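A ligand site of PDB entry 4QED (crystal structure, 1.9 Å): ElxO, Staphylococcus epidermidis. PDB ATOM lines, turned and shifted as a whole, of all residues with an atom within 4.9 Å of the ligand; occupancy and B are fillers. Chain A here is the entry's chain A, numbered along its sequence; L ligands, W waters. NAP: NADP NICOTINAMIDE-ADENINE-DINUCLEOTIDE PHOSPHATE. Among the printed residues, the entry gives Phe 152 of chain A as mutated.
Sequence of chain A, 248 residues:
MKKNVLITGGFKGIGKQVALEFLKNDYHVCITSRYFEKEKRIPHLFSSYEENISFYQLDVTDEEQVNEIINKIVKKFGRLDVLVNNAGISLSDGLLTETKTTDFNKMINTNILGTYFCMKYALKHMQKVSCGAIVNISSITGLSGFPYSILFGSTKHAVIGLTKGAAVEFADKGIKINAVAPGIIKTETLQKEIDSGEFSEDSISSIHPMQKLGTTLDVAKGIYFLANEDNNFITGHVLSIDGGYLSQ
The side-chain hydroxyl of Ser 33 sits at hydrogen-bond distance from an oxygen (O2X) of the ligand, at 2.7 Å.
N of Arg 34 sits at hydrogen-bond distance from O3X of the ligand, 2.9 Å away.
NE of Arg 34 lies within salt-bridge range of O3X of the ligand (2.8 Å).
The backbone NH (N) of Ile 14 is in hydrogen-bond range of an oxygen (O1N) of the ligand.
The side-chain amino group (NZ) of Lys 38 lies within salt-bridge range of an oxygen (O2X) of the ligand (2.8 Å).
The side-chain amino group (NZ) of Lys 156 is in hydrogen-bond range of an oxygen (O3D) of the ligand, 2.9 Å away.
N of Val 60 lies within hydrogen-bond range of N1A of the ligand (2.9 Å).
N of Ile 185 sits at hydrogen-bond distance from O7N of the ligand (3.0 Å).
O of Asn 86 sits at hydrogen-bond distance from O3D of the ligand.
The side-chain carboxylate (OD1) of Asp 59 sits at hydrogen-bond distance from a nitrogen (N6A) of the ligand, at 3.0 Å.
Merely in contact with the ligand: Ser 138, Leu 58, Gly 183, Ile 137, Gly 9, Phe 152, Gly 13, Lys 12, Gly 88, Ala 87, Thr 187, Thr 110, Tyr 35, Pro 182, Ser 139, Ile 184 and Gly 10.
Hydrophobic or aromatic side chains that line the ligand: Ile 14, Tyr 35, Val 60, Ala 87, Ile 137, Phe 152, Pro 182 and Ile 185.
26 residues have an atom within 4 Å of the ligand: Gly 9, Gly 10, Lys 12, Gly 13, Ile 14, Ser 33, Arg 34, Tyr 35, Lys 38, Leu 58, Asp 59, Val 60, Asn 86, Ala 87, Gly 88, Thr 110, Ile 137, Ser 138, Ser 139, Phe 152, Lys 156, Pro 182, Gly 183, Ile 184, Ile 185 and Thr 187.
Water W5 bridges an oxygen (O1X) of the ligand (2.6 Å) and the side-chain amino group of Lys 12 (2.8 Å).
Water W9 lies within hydrogen-bond range of the side-chain hydroxyl of Thr 187 (2.6 Å) and an oxygen (O2N) of the ligand (2.7 Å).
Water W2 lies within hydrogen-bond range of O of Lys 12 (2.6 Å), O3B of the ligand (2.7 Å), N of Gly 10 (2.8 Å) and N of Phe 11 (3.3 Å).
Water W4 lies within hydrogen-bond range of OG1 of Thr 110 (2.6 Å) and N7A of the ligand (2.9 Å).
Water W6 lies within hydrogen-bond range of OG1 of Thr 32 (2.7 Å), O of Leu 58 (2.9 Å), N3A of the ligand (3.0 Å), N of Ser 33 (3.1 Å) and N of Arg 34 (3.4 Å).
Water W11 lies within hydrogen-bond range of O of Ala 87, O3D of the ligand and O of Asn 86.
N of Leu 58 lies within hydrogen-bond range of O of Ser 33 (3.0 Å).
The backbone NH of Tyr 35 lies within hydrogen-bond range of the side-chain hydroxyl of Ser 33 (3.0 Å).
O of Lys 156 is in hydrogen-bond range of OG of Ser 138 (2.8 Å).
N of Asn 86 is in hydrogen-bond range of OG1 of Thr 8 (2.8 Å).
The side-chain carboxylate of Asp 59 sits at hydrogen-bond distance from the side-chain hydroxyl of Thr 61, 2.6 Å away.
The backbone NH of Gly 9 is in hydrogen-bond range of the side-chain hydroxyl of Thr 32, at 2.8 Å.
OE1 of Glu 188 lies within hydrogen-bond range of N of Gly 13.
N of Ala 87 lies within hydrogen-bond range of OG1 of Thr 8, at 2.8 Å.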
ATOM      1  N   THR A   8      22.514  -7.456  11.695  1.00  0.00           N
ATOM      2  CA  THR A   8      22.956  -6.258  11.007  1.00  0.00           C
ATOM      3  C   THR A   8      22.645  -5.072  11.919  1.00  0.00           C
ATOM      4  O   THR A   8      21.543  -4.570  11.943  1.00  0.00           O
ATOM      5  CB  THR A   8      22.333  -6.113   9.616  1.00  0.00           C
ATOM      6  OG1 THR A   8      20.906  -6.052   9.725  1.00  0.00           O
ATOM      7  CG2 THR A   8      22.740  -7.322   8.740  1.00  0.00           C
ATOM      8  N   GLY A   9      23.648  -4.675  12.693  1.00  0.00           N
ATOM      9  CA  GLY A   9      23.461  -3.708  13.775  1.00  0.00           C
ATOM     10  C   GLY A   9      23.874  -4.336  15.093  1.00  0.00           C
ATOM     11  O   GLY A   9      24.621  -5.334  15.114  1.00  0.00           O
ATOM     12  N   GLY A  10      23.382  -3.776  16.193  1.00  0.00           N
ATOM     13  CA  GLY A  10      23.652  -4.315  17.525  1.00  0.00           C
ATOM     14  C   GLY A  10      24.098  -3.270  18.528  1.00  0.00           C
ATOM     15  O   GLY A  10      24.197  -3.563  19.725  1.00  0.00           O
ATOM     16  N   PHE A  11      24.364  -2.054  18.076  1.00  0.00           N
ATOM     17  CA  PHE A  11      24.897  -1.025  18.965  1.00  0.00           C
ATOM     18  C   PHE A  11      23.849  -0.097  19.545  1.00  0.00           C
ATOM     19  O   PHE A  11      24.113   0.598  20.523  1.00  0.00           O
ATOM     20  CB  PHE A  11      26.047  -0.265  18.291  1.00  0.00           C
ATOM     21  CG  PHE A  11      27.324  -1.057  18.221  1.00  0.00           C
ATOM     22  CD1 PHE A  11      27.591  -1.871  17.117  1.00  0.00           C
ATOM     23  CD2 PHE A  11      28.241  -1.015  19.267  1.00  0.00           C
ATOM     24  CE1 PHE A  11      28.758  -2.629  17.066  1.00  0.00           C
ATOM     25  CE2 PHE A  11      29.409  -1.757  19.210  1.00  0.00           C
ATOM     26  CZ  PHE A  11      29.666  -2.567  18.115  1.00  0.00           C
ATOM     27  N   LYS A  12      22.647  -0.096  18.962  1.00  0.00           N
ATOM     28  CA  LYS A  12      21.559   0.773  19.427  1.00  0.00           C
ATOM     29  C   LYS A  12      20.188   0.185  19.093  1.00  0.00           C
ATOM     30  O   LYS A  12      20.089  -0.757  18.308  1.00  0.00           O
ATOM     31  CB  LYS A  12      21.690   2.188  18.832  1.00  0.00           C
ATOM     32  CG  LYS A  12      21.662   2.246  17.306  1.00  0.00           C
ATOM     33  CD  LYS A  12      21.301   3.647  16.816  1.00  0.00           C
ATOM     34  CE  LYS A  12      22.534   4.479  16.523  1.00  0.00           C
ATOM     35  NZ  LYS A  12      22.151   5.735  15.814  1.00  0.00           N
ATOM     36  N   GLY A  13      19.147   0.749  19.683  1.00  0.00           N
ATOM     37  CA  GLY A  13      17.772   0.372  19.376  1.00  0.00           C
ATOM     38  C   GLY A  13      17.450  -1.099  19.520  1.00  0.00           C
ATOM     39  O   GLY A  13      17.983  -1.788  20.399  1.00  0.00           O
ATOM     40  N   ILE A  14      16.574  -1.579  18.638  1.00  0.00           N
ATOM     41  CA  ILE A  14      16.147  -2.973  18.617  1.00  0.00           C
ATOM     42  C   ILE A  14      17.345  -3.944  18.517  1.00  0.00           C
ATOM     43  O   ILE A  14      17.427  -4.929  19.254  1.00  0.00           O
ATOM     44  CB  ILE A  14      15.147  -3.195  17.462  1.00  0.00           C
ATOM     45  CG1 ILE A  14      13.845  -2.417  17.759  1.00  0.00           C
ATOM     46  CG2 ILE A  14      14.851  -4.675  17.263  1.00  0.00           C
ATOM     47  CD1 ILE A  14      12.949  -2.207  16.565  1.00  0.00           C
ATOM     48  N   GLY A  15      18.269  -3.633  17.608  1.00  0.00           N
ATOM     49  CA  GLY A  15      19.444  -4.482  17.378  1.00  0.00           C
ATOM     50  C   GLY A  15      20.265  -4.785  18.616  1.00  0.00           C
ATOM     51  O   GLY A  15      20.728  -5.913  18.799  1.00  0.00           O
ATOM     52  N   THR A  32      27.335  -5.624  14.064  1.00  0.00           N
ATOM     53  CA  THR A  32      27.911  -4.759  13.036  1.00  0.00           C
ATOM     54  C   THR A  32      27.585  -3.287  13.243  1.00  0.00           C
ATOM     55  O   THR A  32      26.598  -2.917  13.895  1.00  0.00           O
ATOM     56  CB  THR A  32      27.480  -5.145  11.587  1.00  0.00           C
ATOM     57  OG1 THR A  32      26.136  -4.729  11.346  1.00  0.00           O
ATOM     58  CG2 THR A  32      27.602  -6.659  11.332  1.00  0.00           C
ATOM     59  N   SER A  33      28.436  -2.450  12.658  1.00  0.00           N
ATOM     60  CA  SER A  33      28.199  -1.016  12.514  1.00  0.00           C
ATOM     61  C   SER A  33      28.916  -0.581  11.246  1.00  0.00           C
ATOM     62  O   SER A  33      29.879  -1.232  10.825  1.00  0.00           O
ATOM     63  CB  SER A  33      28.750  -0.254  13.727  1.00  0.00           C
ATOM     64  OG  SER A  33      28.628   1.139  13.517  1.00  0.00           O
ATOM     65  N   ARG A  34      28.448   0.502  10.647  1.00  0.00           N
ATOM     66  CA  ARG A  34      29.167   1.127   9.539  1.00  0.00           C
ATOM     67  C   ARG A  34      30.445   1.784  10.055  1.00  0.00           C
ATOM     68  O   ARG A  34      31.375   2.058   9.286  1.00  0.00           O
ATOM     69  CB  ARG A  34      28.283   2.167   8.869  1.00  0.00           C
ATOM     70  CG  ARG A  34      27.109   1.590   8.107  1.00  0.00           C
ATOM     71  CD  ARG A  34      26.099   2.681   7.755  1.00  0.00           C
ATOM     72  NE  ARG A  34      25.367   3.142   8.943  1.00  0.00           N
ATOM     73  CZ  ARG A  34      24.443   4.089   8.916  1.00  0.00           C
ATOM     74  NH1 ARG A  34      24.100   4.687   7.772  1.00  0.00           N
ATOM     75  NH2 ARG A  34      23.832   4.437  10.043  1.00  0.00           N
ATOM     76  N   TYR A  35      30.491   2.014  11.372  1.00  0.00           N
ATOM     77  CA  TYR A  35      31.528   2.829  12.007  1.00  0.00           C
ATOM     78  C   TYR A  35      32.457   1.966  12.854  1.00  0.00           C
ATOM     79  O   TYR A  35      32.043   1.432  13.874  1.00  0.00           O
ATOM     80  CB  TYR A  35      30.874   3.920  12.862  1.00  0.00           C
ATOM     81  CG  TYR A  35      29.935   4.798  12.084  1.00  0.00           C
ATOM     82  CD1 TYR A  35      30.422   5.886  11.341  1.00  0.00           C
ATOM     83  CD2 TYR A  35      28.565   4.531  12.048  1.00  0.00           C
ATOM     84  CE1 TYR A  35      29.562   6.678  10.597  1.00  0.00           C
ATOM     85  CE2 TYR A  35      27.705   5.323  11.304  1.00  0.00           C
ATOM     86  CZ  TYR A  35      28.210   6.402  10.583  1.00  0.00           C
ATOM     87  OH  TYR A  35      27.364   7.195   9.843  1.00  0.00           O
ATOM     88  N   LYS A  38      32.923   2.091  16.803  1.00  0.00           N
ATOM     89  CA  LYS A  38      31.975   1.522  17.751  1.00  0.00           C
ATOM     90  C   LYS A  38      32.511   0.260  18.433  1.00  0.00           C
ATOM     91  O   LYS A  38      32.082  -0.077  19.537  1.00  0.00           O
ATOM     92  CB  LYS A  38      30.603   1.294  17.106  1.00  0.00           C
ATOM     93  CG  LYS A  38      29.906   2.593  16.710  1.00  0.00           C
ATOM     94  CD  LYS A  38      28.395   2.430  16.587  1.00  0.00           C
ATOM     95  CE  LYS A  38      27.757   3.697  16.053  1.00  0.00           C
ATOM     96  NZ  LYS A  38      26.278   3.578  15.870  1.00  0.00           N
ATOM     97  N   LEU A  58      30.386  -3.078   8.570  1.00  0.00           N
ATOM     98  CA  LEU A  58      29.530  -3.488   7.464  1.00  0.00           C
ATOM     99  C   LEU A  58      28.517  -2.411   7.094  1.00  0.00           C
ATOM    100  O   LEU A  58      27.796  -1.914   7.956  1.00  0.00           O
ATOM    101  CB  LEU A  58      28.764  -4.792   7.808  1.00  0.00           C
ATOM    102  CG  LEU A  58      27.785  -5.311   6.736  1.00  0.00           C
ATOM    103  CD1 LEU A  58      28.506  -5.777   5.474  1.00  0.00           C
ATOM    104  CD2 LEU A  58      26.890  -6.406   7.295  1.00  0.00           C
ATOM    105  N   ASP A  59      28.490  -2.052   5.818  1.00  0.00           N
ATOM    106  CA  ASP A  59      27.376  -1.304   5.263  1.00  0.00           C
ATOM    107  C   ASP A  59      26.554  -2.282   4.432  1.00  0.00           C
ATOM    108  O   ASP A  59      27.061  -2.842   3.454  1.00  0.00           O
ATOM    109  CB  ASP A  59      27.862  -0.137   4.409  1.00  0.00           C
ATOM    110  CG  ASP A  59      26.758   0.854   4.086  1.00  0.00           C
ATOM    111  OD1 ASP A  59      25.639   0.426   3.707  1.00  0.00           O
ATOM    112  OD2 ASP A  59      27.001   2.068   4.211  1.00  0.00           O
ATOM    113  N   VAL A  60      25.298  -2.500   4.809  1.00  0.00           N
ATOM    114  CA  VAL A  60      24.435  -3.477   4.116  1.00  0.00           C
ATOM    115  C   VAL A  60      24.087  -3.081   2.675  1.00  0.00           C
ATOM    116  O   VAL A  60      23.667  -3.944   1.891  1.00  0.00           O
ATOM    117  CB  VAL A  60      23.145  -3.837   4.924  1.00  0.00           C
ATOM    118  CG1 VAL A  60      23.501  -4.472   6.269  1.00  0.00           C
ATOM    119  CG2 VAL A  60      22.224  -2.641   5.096  1.00  0.00           C
ATOM    120  N   THR A  61      24.280  -1.816   2.328  1.00  0.00           N
ATOM    121  CA  THR A  61      24.050  -1.370   0.951  1.00  0.00           C
ATOM    122  C   THR A  61      25.203  -1.725   0.006  1.00  0.00           C
ATOM    123  O   THR A  61      25.087  -1.549  -1.202  1.00  0.00           O
ATOM    124  CB  THR A  61      23.780   0.146   0.854  1.00  0.00           C
ATOM    125  OG1 THR A  61      24.958   0.882   1.242  1.00  0.00           O
ATOM    126  CG2 THR A  61      22.592   0.539   1.724  1.00  0.00           C
ATOM    127  N   ASN A  86      18.334  -6.510  10.821  1.00  0.00           N
ATOM    128  CA  ASN A  86      17.898  -5.403  11.676  1.00  0.00           C
ATOM    129  C   ASN A  86      18.107  -4.030  11.043  1.00  0.00           C
ATOM    130  O   ASN A  86      17.259  -3.154  11.180  1.00  0.00           O
ATOM    131  CB  ASN A  86      18.590  -5.499  13.035  1.00  0.00           C
ATOM    132  CG  ASN A  86      18.413  -4.254  13.883  1.00  0.00           C
ATOM    133  OD1 ASN A  86      19.319  -3.408  13.966  1.00  0.00           O
ATOM    134  ND2 ASN A  86      17.242  -4.124  14.505  1.00  0.00           N
ATOM    135  N   ALA A  87      19.231  -3.851  10.350  1.00  0.00           N
ATOM    136  CA  ALA A  87      19.570  -2.584   9.705  1.00  0.00           C
ATOM    137  C   ALA A  87      18.377  -1.989   8.959  1.00  0.00           C
ATOM    138  O   ALA A  87      17.773  -2.652   8.109  1.00  0.00           O
ATOM    139  CB  ALA A  87      20.747  -2.770   8.747  1.00  0.00           C
ATOM    140  N   GLY A  88      18.015  -0.751   9.279  1.00  0.00           N
ATOM    141  CA  GLY A  88      16.921  -0.096   8.590  1.00  0.00           C
ATOM    142  C   GLY A  88      16.787   1.359   8.976  1.00  0.00           C
ATOM    143  O   GLY A  88      17.162   1.750  10.083  1.00  0.00           O
ATOM    144  N   ILE A  89      16.257   2.153   8.046  1.00  0.00           N
ATOM    145  CA  ILE A  89      16.132   3.597   8.221  1.00  0.00           C
ATOM    146  C   ILE A  89      14.750   4.099   7.806  1.00  0.00           C
ATOM    147  O   ILE A  89      14.088   3.527   6.921  1.00  0.00           O
ATOM    148  CB  ILE A  89      17.206   4.398   7.449  1.00  0.00           C
ATOM    149  CG1 ILE A  89      17.217   4.014   5.955  1.00  0.00           C
ATOM    150  CG2 ILE A  89      18.589   4.192   8.084  1.00  0.00           C
ATOM    151  CD1 ILE A  89      18.066   4.920   5.082  1.00  0.00           C
ATOM    152  N   THR A 110      18.816   0.625   1.781  1.00  0.00           N
ATOM    153  CA  THR A 110      19.075   0.038   3.088  1.00  0.00           C
ATOM    154  C   THR A 110      18.030  -1.027   3.443  1.00  0.00           C
ATOM    155  O   THR A 110      18.385  -2.163   3.772  1.00  0.00           O
ATOM    156  CB  THR A 110      19.142   1.111   4.194  1.00  0.00           C
ATOM    157  OG1 THR A 110      20.195   2.028   3.888  1.00  0.00           O
ATOM    158  CG2 THR A 110      19.420   0.464   5.567  1.00  0.00           C
ATOM    159  N   ILE A 137      13.020  -7.706   9.680  1.00  0.00           N
ATOM    160  CA  ILE A 137      12.203  -6.756  10.411  1.00  0.00           C
ATOM    161  C   ILE A 137      11.420  -5.881   9.445  1.00  0.00           C
ATOM    162  O   ILE A 137      11.992  -5.104   8.675  1.00  0.00           O
ATOM    163  CB  ILE A 137      13.016  -5.897  11.412  1.00  0.00           C
ATOM    164  CG1 ILE A 137      13.776  -6.801  12.396  1.00  0.00           C
ATOM    165  CG2 ILE A 137      12.094  -4.930  12.152  1.00  0.00           C
ATOM    166  CD1 ILE A 137      14.600  -6.034  13.415  1.00  0.00           C
ATOM    167  N   SER A 138      10.102  -6.059   9.460  1.00  0.00           N
ATOM    168  CA  SER A 138       9.208  -5.226   8.694  1.00  0.00           C
ATOM    169  C   SER A 138       8.666  -4.146   9.631  1.00  0.00           C
ATOM    170  O   SER A 138       9.432  -3.519  10.367  1.00  0.00           O
ATOM    171  CB  SER A 138       8.097  -6.061   8.066  1.00  0.00           C
ATOM    172  OG  SER A 138       7.298  -5.272   7.195  1.00  0.00           O
ATOM    173  N   SER A 139       7.353  -3.941   9.608  1.00  0.00           N
ATOM    174  CA  SER A 139       6.689  -2.895  10.397  1.00  0.00           C
ATOM    175  C   SER A 139       5.190  -3.060  10.224  1.00  0.00           C
ATOM    176  O   SER A 139       4.741  -3.693   9.269  1.00  0.00           O
ATOM    177  CB  SER A 139       7.127  -1.511   9.874  1.00  0.00           C
ATOM    178  OG  SER A 139       6.268  -0.463  10.293  1.00  0.00           O
ATOM    179  N   PHE A 152       8.414   4.654   3.541  1.00  0.00           N
ATOM    180  CA  PHE A 152       8.937   3.698   4.499  1.00  0.00           C
ATOM    181  C   PHE A 152       8.096   2.417   4.484  1.00  0.00           C
ATOM    182  O   PHE A 152       8.639   1.302   4.424  1.00  0.00           O
ATOM    183  CB  PHE A 152       8.948   4.289   5.919  1.00  0.00           C
ATOM    184  CG  PHE A 152       9.402   3.325   6.979  1.00  0.00           C
ATOM    185  CD1 PHE A 152       8.482   2.763   7.869  1.00  0.00           C
ATOM    186  CD2 PHE A 152      10.746   2.958   7.082  1.00  0.00           C
ATOM    187  CE1 PHE A 152       8.891   1.873   8.850  1.00  0.00           C
ATOM    188  CE2 PHE A 152      11.168   2.070   8.066  1.00  0.00           C
ATOM    189  CZ  PHE A 152      10.243   1.527   8.942  1.00  0.00           C
ATOM    190  N   LYS A 156       8.926  -1.612   3.663  1.00  0.00           N
ATOM    191  CA  LYS A 156       8.636  -2.682   4.609  1.00  0.00           C
ATOM    192  C   LYS A 156       7.645  -3.718   4.042  1.00  0.00           C
ATOM    193  O   LYS A 156       7.676  -4.873   4.452  1.00  0.00           O
ATOM    194  CB  LYS A 156       8.211  -2.126   5.976  1.00  0.00           C
ATOM    195  CG  LYS A 156       9.319  -1.359   6.696  1.00  0.00           C
ATOM    196  CD  LYS A 156      10.599  -2.184   6.836  1.00  0.00           C
ATOM    197  CE  LYS A 156      11.533  -1.619   7.896  1.00  0.00           C
ATOM    198  NZ  LYS A 156      12.729  -2.482   8.124  1.00  0.00           N
ATOM    199  N   PRO A 182       6.897  -4.679  13.905  1.00  0.00           N
ATOM    200  CA  PRO A 182       6.716  -3.881  15.108  1.00  0.00           C
ATOM    201  C   PRO A 182       5.803  -2.682  14.889  1.00  0.00           C
ATOM    202  O   PRO A 182       5.759  -2.125  13.791  1.00  0.00           O
ATOM    203  CB  PRO A 182       8.142  -3.413  15.442  1.00  0.00           C
ATOM    204  CG  PRO A 182       9.062  -4.288  14.651  1.00  0.00           C
ATOM    205  CD  PRO A 182       8.285  -4.614  13.400  1.00  0.00           C
ATOM    206  N   GLY A 183       5.051  -2.325  15.927  1.00  0.00           N
ATOM    207  CA  GLY A 183       4.385  -1.021  16.003  1.00  0.00           C
ATOM    208  C   GLY A 183       5.440   0.019  16.336  1.00  0.00           C
ATOM    209  O   GLY A 183       6.620  -0.160  15.992  1.00  0.00           O
ATOM    210  N   ILE A 184       5.051   1.111  17.001  1.00  0.00           N
ATOM    211  CA  ILE A 184       6.021   2.148  17.384  1.00  0.00           C
ATOM    212  C   ILE A 184       6.785   1.690  18.639  1.00  0.00           C
ATOM    213  O   ILE A 184       6.175   1.380  19.666  1.00  0.00           O
ATOM    214  CB  ILE A 184       5.355   3.526  17.612  1.00  0.00           C
ATOM    215  CG1 ILE A 184       4.642   3.978  16.329  1.00  0.00           C
ATOM    216  CG2 ILE A 184       6.397   4.558  18.032  1.00  0.00           C
ATOM    217  CD1 ILE A 184       3.784   5.216  16.497  1.00  0.00           C
ATOM    218  N   ILE A 185       8.106   1.624  18.515  1.00  0.00           N
ATOM    219  CA  ILE A 185       8.959   1.062  19.564  1.00  0.00           C
ATOM    220  C   ILE A 185       9.763   2.177  20.242  1.00  0.00           C
ATOM    221  O   ILE A 185      10.379   3.012  19.570  1.00  0.00           O
ATOM    222  CB  ILE A 185       9.935  -0.013  19.002  1.00  0.00           C
ATOM    223  CG1 ILE A 185       9.179  -1.111  18.215  1.00  0.00           C
ATOM    224  CG2 ILE A 185      10.813  -0.591  20.104  1.00  0.00           C
ATOM    225  CD1 ILE A 185       8.050  -1.815  18.964  1.00  0.00           C
ATOM    226  N   THR A 187      12.728   3.295  21.342  1.00  0.00           N
ATOM    227  CA  THR A 187      14.177   3.195  21.305  1.00  0.00           C
ATOM    228  C   THR A 187      14.797   4.427  21.975  1.00  0.00           C
ATOM    229  O   THR A 187      14.077   5.375  22.338  1.00  0.00           O
ATOM    230  CB  THR A 187      14.667   3.139  19.851  1.00  0.00           C
ATOM    231  OG1 THR A 187      14.219   4.314  19.171  1.00  0.00           O
ATOM    232  CG2 THR A 187      14.130   1.887  19.148  1.00  0.00           C
ATOM    233  N   GLU A 188      16.126   4.423  22.125  1.00  0.00           N
ATOM    234  CA  GLU A 188      16.876   5.593  22.616  1.00  0.00           C
ATOM    235  C   GLU A 188      16.531   6.867  21.832  1.00  0.00           C
ATOM    236  O   GLU A 188      16.282   7.924  22.414  1.00  0.00           O
ATOM    237  CB  GLU A 188      18.401   5.363  22.585  1.00  0.00           C
ATOM    238  CG  GLU A 188      18.890   4.106  23.279  1.00  0.00           C
ATOM    239  CD  GLU A 188      19.167   2.956  22.315  1.00  0.00           C
ATOM    240  OE1 GLU A 188      18.713   3.036  21.152  1.00  0.00           O
ATOM    241  OE2 GLU A 188      19.834   1.983  22.714  1.00  0.00           O
ATOM    242  N   THR A 189      16.524   6.737  20.502  1.00  0.00           N
ATOM    243  CA  THR A 189      16.188   7.837  19.596  1.00  0.00           C
ATOM    244  C   THR A 189      14.814   8.451  19.917  1.00  0.00           C
ATOM    245  O   THR A 189      14.677   9.665  20.014  1.00  0.00           O
ATOM    246  CB  THR A 189      16.253   7.388  18.112  1.00  0.00           C
ATOM    247  OG1 THR A 189      17.527   6.791  17.862  1.00  0.00           O
ATOM    248  CG2 THR A 189      16.055   8.553  17.155  1.00  0.00           C
HETATM  249  PA  NAP L   1      18.058   2.542  15.082  1.00  0.00           P
HETATM  250  O1A NAP L   1      18.036   2.548  16.582  1.00  0.00           O
HETATM  251  O2A NAP L   1      18.036   3.780  14.249  1.00  0.00           O
HETATM  252  O5B NAP L   1      19.396   1.766  14.640  1.00  0.00           O
HETATM  253  C5B NAP L   1      19.676   1.552  13.265  1.00  0.00           C
HETATM  254  C4B NAP L   1      20.616   0.349  13.170  1.00  0.00           C
HETATM  255  O4B NAP L   1      20.733   0.016  11.789  1.00  0.00           O
HETATM  256  C3B NAP L   1      22.010   0.696  13.649  1.00  0.00           C
HETATM  257  O3B NAP L   1      22.575  -0.473  14.269  1.00  0.00           O
HETATM  258  C2B NAP L   1      22.767   1.011  12.378  1.00  0.00           C
HETATM  259  O2B NAP L   1      24.162   0.768  12.494  1.00  0.00           O
HETATM  260  C1B NAP L   1      22.106   0.065  11.383  1.00  0.00           C
HETATM  261  N9A NAP L   1      22.215   0.542   9.986  1.00  0.00           N
HETATM  262  C8A NAP L   1      21.536   1.555   9.440  1.00  0.00           C
HETATM  263  N7A NAP L   1      21.898   1.680   8.149  1.00  0.00           N
HETATM  264  C5A NAP L   1      22.829   0.734   7.905  1.00  0.00           C
HETATM  265  C6A NAP L   1      23.545   0.394   6.768  1.00  0.00           C
HETATM  266  N6A NAP L   1      23.369   1.094   5.620  1.00  0.00           N
HETATM  267  N1A NAP L   1      24.411  -0.646   6.826  1.00  0.00           N
HETATM  268  C2A NAP L   1      24.579  -1.335   7.972  1.00  0.00           C
HETATM  269  N3A NAP L   1      23.895  -1.030   9.082  1.00  0.00           N
HETATM  270  C4A NAP L   1      23.013   0.007   9.062  1.00  0.00           C
HETATM  271  O3  NAP L   1      16.949   1.548  14.478  1.00  0.00           O
HETATM  272  PN  NAP L   1      15.720   0.857  15.243  1.00  0.00           P
HETATM  273  O1N NAP L   1      16.162  -0.034  16.357  1.00  0.00           O
HETATM  274  O2N NAP L   1      14.637   1.884  15.453  1.00  0.00           O
HETATM  275  O5D NAP L   1      15.216  -0.066  14.018  1.00  0.00           O
HETATM  276  C5D NAP L   1      15.726  -1.369  13.743  1.00  0.00           C
HETATM  277  C4D NAP L   1      14.854  -1.999  12.659  1.00  0.00           C
HETATM  278  O4D NAP L   1      13.498  -2.036  13.111  1.00  0.00           O
HETATM  279  C3D NAP L   1      14.836  -1.219  11.345  1.00  0.00           C
HETATM  280  O3D NAP L   1      14.636  -2.137  10.248  1.00  0.00           O
HETATM  281  C2D NAP L   1      13.596  -0.348  11.474  1.00  0.00           C
HETATM  282  O2D NAP L   1      13.114   0.105  10.201  1.00  0.00           O
HETATM  283  C1D NAP L   1      12.666  -1.344  12.170  1.00  0.00           C
HETATM  284  N1N NAP L   1      11.517  -0.743  12.833  1.00  0.00           N
HETATM  285  C2N NAP L   1      11.670   0.166  13.829  1.00  0.00           C
HETATM  286  C3N NAP L   1      10.539   0.724  14.432  1.00  0.00           C
HETATM  287  C7N NAP L   1      10.631   1.738  15.546  1.00  0.00           C
HETATM  288  O7N NAP L   1       9.594   2.169  16.023  1.00  0.00           O
HETATM  289  N7N NAP L   1      11.820   2.159  16.002  1.00  0.00           N
HETATM  290  C4N NAP L   1       9.275   0.312  14.011  1.00  0.00           C
HETATM  291  C5N NAP L   1       9.146  -0.638  12.993  1.00  0.00           C
HETATM  292  C6N NAP L   1      10.296  -1.160  12.417  1.00  0.00           C
HETATM  293  P2B NAP L   1      25.253   1.973  12.591  1.00  0.00           P
HETATM  294  O1X NAP L   1      24.459   3.257  12.690  1.00  0.00           O
HETATM  295  O2X NAP L   1      26.049   1.657  13.842  1.00  0.00           O
HETATM  296  O3X NAP L   1      26.015   1.857  11.302  1.00  0.00           O
HETATM  297  O   HOH W   1      17.853   4.367  18.656  1.00  0.00           O
HETATM  298  O   HOH W   2      21.547  -1.735  16.392  1.00  0.00           O
HETATM  299  O   HOH W   3      14.226   3.406  13.054  1.00  0.00           O
HETATM  300  O   HOH W   4      21.370   3.310   5.860  1.00  0.00           O
HETATM  301  O   HOH W   5      22.248   4.530  13.272  1.00  0.00           O
HETATM  302  O   HOH W   6      26.287  -2.177  10.468  1.00  0.00           O
HETATM  303  O   HOH W   7      18.576  -1.333  15.701  1.00  0.00           O
HETATM  304  O   HOH W   8      17.649   3.837  11.532  1.00  0.00           O
HETATM  305  O   HOH W   9      14.616   4.304  16.555  1.00  0.00           O
HETATM  306  O   HOH W  10      12.807   2.706  10.975  1.00  0.00           O
HETATM  307  O   HOH W  11      15.713  -4.370   8.548  1.00  0.00           O
HETATM  308  O   HOH W  12      19.469   6.202  14.543  1.00  0.00           O
HETATM  309  O   HOH W  13      10.262   4.809  17.305  1.00  0.00           O
HETATM  310  O   HOH W  14      25.231   5.469  14.240  1.00  0.00           O
HETATM  311  O   HOH W  15      25.109  -0.705  14.982  1.00  0.00           O
HETATM  312  O   HOH W  16       8.264   4.163  14.467  1.00  0.00           O
